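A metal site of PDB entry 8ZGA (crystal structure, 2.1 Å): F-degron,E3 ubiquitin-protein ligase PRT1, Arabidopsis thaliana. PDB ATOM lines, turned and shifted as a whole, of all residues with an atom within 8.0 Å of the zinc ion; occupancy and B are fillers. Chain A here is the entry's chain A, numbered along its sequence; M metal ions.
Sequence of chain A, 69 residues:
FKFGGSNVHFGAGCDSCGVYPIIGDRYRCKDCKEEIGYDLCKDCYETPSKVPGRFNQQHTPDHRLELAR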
ATOM      1  N   GLY A  13      23.867   6.342 -17.424  1.00  0.00           N
ATOM      2  CA  GLY A  13      23.651   5.182 -16.594  1.00  0.00           C
ATOM      3  C   GLY A  13      24.792   4.997 -15.617  1.00  0.00           C
ATOM      4  O   GLY A  13      25.915   5.448 -15.836  1.00  0.00           O
ATOM      5  N   CYS A  14      24.477   4.326 -14.501  1.00  0.00           N
ATOM      6  CA  CYS A  14      25.453   4.109 -13.452  1.00  0.00           C
ATOM      7  C   CYS A  14      26.345   2.916 -13.805  1.00  0.00           C
ATOM      8  O   CYS A  14      25.845   1.856 -14.181  1.00  0.00           O
ATOM      9  CB  CYS A  14      24.755   3.870 -12.117  1.00  0.00           C
ATOM     10  SG  CYS A  14      25.871   3.535 -10.728  1.00  0.00           S
ATOM     11  N   ASP A  15      27.653   3.096 -13.663  1.00  0.00           N
ATOM     12  CA  ASP A  15      28.615   2.051 -14.014  1.00  0.00           C
ATOM     13  C   ASP A  15      28.771   0.978 -12.940  1.00  0.00           C
ATOM     14  O   ASP A  15      29.510   0.008 -13.170  1.00  0.00           O
ATOM     15  CB  ASP A  15      29.978   2.696 -14.301  1.00  0.00           C
ATOM     16  CG  ASP A  15      30.083   3.234 -15.708  1.00  0.00           C
ATOM     17  OD1 ASP A  15      30.226   2.437 -16.655  1.00  0.00           O
ATOM     18  OD2 ASP A  15      30.047   4.475 -15.876  1.00  0.00           O
ATOM     19  N   SER A  16      28.094   1.103 -11.798  1.00  0.00           N
ATOM     20  CA  SER A  16      28.138   0.115 -10.736  1.00  0.00           C
ATOM     21  C   SER A  16      26.866  -0.718 -10.631  1.00  0.00           C
ATOM     22  O   SER A  16      26.945  -1.954 -10.675  1.00  0.00           O
ATOM     23  CB  SER A  16      28.433   0.804  -9.392  1.00  0.00           C
ATOM     24  OG  SER A  16      27.227   1.201  -8.757  1.00  0.00           O
ATOM     25  N   CYS A  17      25.698  -0.075 -10.523  1.00  0.00           N
ATOM     26  CA  CYS A  17      24.411  -0.761 -10.472  1.00  0.00           C
ATOM     27  C   CYS A  17      23.754  -0.929 -11.843  1.00  0.00           C
ATOM     28  O   CYS A  17      22.934  -1.843 -12.011  1.00  0.00           O
ATOM     29  CB  CYS A  17      23.441   0.000  -9.551  1.00  0.00           C
ATOM     30  SG  CYS A  17      22.879   1.607 -10.135  1.00  0.00           S
ATOM     31  N   GLY A  18      24.078  -0.079 -12.820  1.00  0.00           N
ATOM     32  CA  GLY A  18      23.543  -0.216 -14.162  1.00  0.00           C
ATOM     33  C   GLY A  18      22.215   0.471 -14.406  1.00  0.00           C
ATOM     34  O   GLY A  18      21.627   0.298 -15.489  1.00  0.00           O
ATOM     35  N   VAL A  19      21.715   1.227 -13.436  1.00  0.00           N
ATOM     36  CA  VAL A  19      20.447   1.910 -13.609  1.00  0.00           C
ATOM     37  C   VAL A  19      20.551   2.870 -14.778  1.00  0.00           C
ATOM     38  O   VAL A  19      21.557   3.577 -14.948  1.00  0.00           O
ATOM     39  CB  VAL A  19      20.051   2.636 -12.308  1.00  0.00           C
ATOM     40  CG1 VAL A  19      21.043   3.739 -11.993  1.00  0.00           C
ATOM     41  CG2 VAL A  19      18.641   3.207 -12.449  1.00  0.00           C
ATOM     42  N   ILE A  22      19.814   7.494 -14.986  1.00  0.00           N
ATOM     43  CA  ILE A  22      20.087   7.770 -13.575  1.00  0.00           C
ATOM     44  C   ILE A  22      19.005   8.696 -13.036  1.00  0.00           C
ATOM     45  O   ILE A  22      18.774   9.778 -13.586  1.00  0.00           O
ATOM     46  CB  ILE A  22      21.483   8.374 -13.390  1.00  0.00           C
ATOM     47  CG1 ILE A  22      22.555   7.345 -13.759  1.00  0.00           C
ATOM     48  CG2 ILE A  22      21.676   8.856 -11.947  1.00  0.00           C
ATOM     49  CD1 ILE A  22      23.982   7.829 -13.620  1.00  0.00           C
ATOM     50  N   ASP A  25      20.655  12.471  -8.182  1.00  0.00           N
ATOM     51  CA  ASP A  25      21.948  13.092  -8.432  1.00  0.00           C
ATOM     52  C   ASP A  25      22.867  12.130  -9.186  1.00  0.00           C
ATOM     53  O   ASP A  25      22.794  10.908  -9.040  1.00  0.00           O
ATOM     54  CB  ASP A  25      22.606  13.528  -7.123  1.00  0.00           C
ATOM     55  CG  ASP A  25      21.928  14.727  -6.512  1.00  0.00           C
ATOM     56  OD1 ASP A  25      21.310  15.519  -7.262  1.00  0.00           O
ATOM     57  OD2 ASP A  25      22.001  14.894  -5.278  1.00  0.00           O
ATOM     58  N   ASP A  39      30.112   7.438 -15.204  1.00  0.00           N
ATOM     59  CA  ASP A  39      29.095   8.033 -14.343  1.00  0.00           C
ATOM     60  C   ASP A  39      28.730   7.064 -13.229  1.00  0.00           C
ATOM     61  O   ASP A  39      28.869   5.846 -13.369  1.00  0.00           O
ATOM     62  CB  ASP A  39      27.840   8.407 -15.133  1.00  0.00           C
ATOM     63  CG  ASP A  39      28.143   9.341 -16.293  1.00  0.00           C
ATOM     64  OD1 ASP A  39      28.610   8.860 -17.338  1.00  0.00           O
ATOM     65  OD2 ASP A  39      27.908  10.562 -16.138  1.00  0.00           O
ATOM     66  N   LEU A  40      28.250   7.628 -12.124  1.00  0.00           N
ATOM     67  CA  LEU A  40      27.779   6.860 -10.986  1.00  0.00           C
ATOM     68  C   LEU A  40      26.566   7.550 -10.399  1.00  0.00           C
ATOM     69  O   LEU A  40      26.464   8.774 -10.394  1.00  0.00           O
ATOM     70  CB  LEU A  40      28.869   6.721  -9.912  1.00  0.00           C
ATOM     71  CG  LEU A  40      30.083   5.849 -10.247  1.00  0.00           C
ATOM     72  CD1 LEU A  40      31.095   5.906  -9.121  1.00  0.00           C
ATOM     73  CD2 LEU A  40      29.643   4.418 -10.511  1.00  0.00           C
ATOM     74  N   CYS A  41      25.640   6.744  -9.880  1.00  0.00           N
ATOM     75  CA  CYS A  41      24.513   7.275  -9.130  1.00  0.00           C
ATOM     76  C   CYS A  41      24.951   7.636  -7.713  1.00  0.00           C
ATOM     77  O   CYS A  41      26.083   7.361  -7.281  1.00  0.00           O
ATOM     78  CB  CYS A  41      23.356   6.266  -9.108  1.00  0.00           C
ATOM     79  SG  CYS A  41      23.559   4.858  -8.013  1.00  0.00           S
ATOM     80  N   LYS A  42      24.044   8.271  -6.974  1.00  0.00           N
ATOM     81  CA  LYS A  42      24.455   8.891  -5.728  1.00  0.00           C
ATOM     82  C   LYS A  42      24.656   7.844  -4.627  1.00  0.00           C
ATOM     83  O   LYS A  42      25.671   7.886  -3.916  1.00  0.00           O
ATOM     84  CB  LYS A  42      23.433   9.973  -5.313  1.00  0.00           C
ATOM     85  CG  LYS A  42      23.600  10.435  -3.873  1.00  0.00           C
ATOM     86  CD  LYS A  42      22.400  11.234  -3.383  1.00  0.00           C
ATOM     87  CE  LYS A  42      22.642  11.842  -2.019  1.00  0.00           C
ATOM     88  NZ  LYS A  42      21.425  12.595  -1.607  1.00  0.00           N
ATOM     89  N   ASP A  43      23.758   6.868  -4.490  1.00  0.00           N
ATOM     90  CA  ASP A  43      23.949   5.798  -3.502  1.00  0.00           C
ATOM     91  C   ASP A  43      25.238   4.998  -3.764  1.00  0.00           C
ATOM     92  O   ASP A  43      26.036   4.767  -2.851  1.00  0.00           O
ATOM     93  CB  ASP A  43      22.743   4.857  -3.462  1.00  0.00           C
ATOM     94  CG  ASP A  43      21.420   5.616  -3.364  1.00  0.00           C
ATOM     95  OD1 ASP A  43      21.445   6.784  -2.902  1.00  0.00           O
ATOM     96  OD2 ASP A  43      20.372   5.051  -3.740  1.00  0.00           O
ATOM     97  N   CYS A  44      25.463   4.585  -5.025  1.00  0.00           N
ATOM     98  CA  CYS A  44      26.726   3.925  -5.399  1.00  0.00           C
ATOM     99  C   CYS A  44      27.941   4.831  -5.183  1.00  0.00           C
ATOM    100  O   CYS A  44      28.986   4.358  -4.721  1.00  0.00           O
ATOM    101  CB  CYS A  44      26.672   3.455  -6.855  1.00  0.00           C
ATOM    102  SG  CYS A  44      25.369   2.232  -7.128  1.00  0.00           S
ATOM    103  N   TYR A  45      27.803   6.135  -5.486  1.00  0.00           N
ATOM    104  CA  TYR A  45      28.880   7.097  -5.186  1.00  0.00           C
ATOM    105  C   TYR A  45      29.240   7.079  -3.693  1.00  0.00           C
ATOM    106  O   TYR A  45      30.395   6.853  -3.310  1.00  0.00           O
ATOM    107  CB  TYR A  45      28.467   8.511  -5.633  1.00  0.00           C
ATOM    108  CG  TYR A  45      29.570   9.534  -5.442  1.00  0.00           C
ATOM    109  CD1 TYR A  45      30.779   9.394  -6.095  1.00  0.00           C
ATOM    110  CD2 TYR A  45      29.412  10.640  -4.595  1.00  0.00           C
ATOM    111  CE1 TYR A  45      31.816  10.298  -5.911  1.00  0.00           C
ATOM    112  CE2 TYR A  45      30.453  11.558  -4.409  1.00  0.00           C
ATOM    113  CZ  TYR A  45      31.657  11.382  -5.070  1.00  0.00           C
ATOM    114  OH  TYR A  45      32.675  12.285  -4.875  1.00  0.00           O
ATOM    115  N   VAL A  51      34.759   0.106  -9.071  1.00  0.00           N
ATOM    116  CA  VAL A  51      33.942   0.139 -10.285  1.00  0.00           C
ATOM    117  C   VAL A  51      34.858   0.607 -11.428  1.00  0.00           C
ATOM    118  O   VAL A  51      34.919   1.796 -11.738  1.00  0.00           O
ATOM    119  CB  VAL A  51      32.709   1.047 -10.110  1.00  0.00           C
ATOM    120  CG1 VAL A  51      31.818   1.025 -11.342  1.00  0.00           C
ATOM    121  CG2 VAL A  51      31.887   0.635  -8.874  1.00  0.00           C
ATOM    122  N   ARG A  54      31.737  -0.403 -17.033  1.00  0.00           N
ATOM    123  CA  ARG A  54      31.129  -1.478 -17.814  1.00  0.00           C
ATOM    124  C   ARG A  54      31.491  -1.445 -19.292  1.00  0.00           C
ATOM    125  O   ARG A  54      31.198  -2.427 -20.001  1.00  0.00           O
ATOM    126  CB  ARG A  54      29.605  -1.395 -17.692  1.00  0.00           C
ATOM    127  CG  ARG A  54      29.106  -1.314 -16.272  1.00  0.00           C
ATOM    128  CD  ARG A  54      27.593  -1.212 -16.238  1.00  0.00           C
ATOM    129  NE  ARG A  54      27.056  -1.530 -14.911  1.00  0.00           N
ATOM    130  CZ  ARG A  54      26.800  -2.758 -14.497  1.00  0.00           C
ATOM    131  NH1 ARG A  54      26.303  -2.959 -13.282  1.00  0.00           N
ATOM    132  NH2 ARG A  54      27.026  -3.795 -15.292  1.00  0.00           N
HETATM  133 ZN    ZN M   1      24.360   3.085  -9.151  1.00  0.00          ZN
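The side-chain sulfur (SG) of Cys 17 lies close to the backbone NH (N) of Val 19, at 3.5 Å.
SG of Cys 44 lies close to OG of Ser 16.
The side-chain sulfur (SG) of Cys 14 lies close to the side-chain hydroxyl (OG) of Ser 16.
O of Val 19 lies within hydrogen-bond range of N of Cys 14 (3.0 Å).
O of Ser 16 lies within hydrogen-bond range of NH1 of Arg 54 (2.9 Å).
Residues that only touch the zinc ion: Ser 16 (3.5 Å).
Five residues have an atom within 4 Å of the zinc ion: Cys 14, Ser 16, Cys 17, Cys 41 and Cys 44.
The nearest printed residue that does not touch the zinc ion is Val 19 (4.4 Å).
The zinc ion is bound by the side-chain sulfur (SG) of Cys 14 (2.2 Å), the side-chain sulfur (SG) of Cys 41 (2.3 Å), the side-chain sulfur (SG) of Cys 17 (2.3 Å) and the side-chain sulfur (SG) of Cys 44 (2.4 Å).
The zinc ion has four donor atoms within binding distance.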
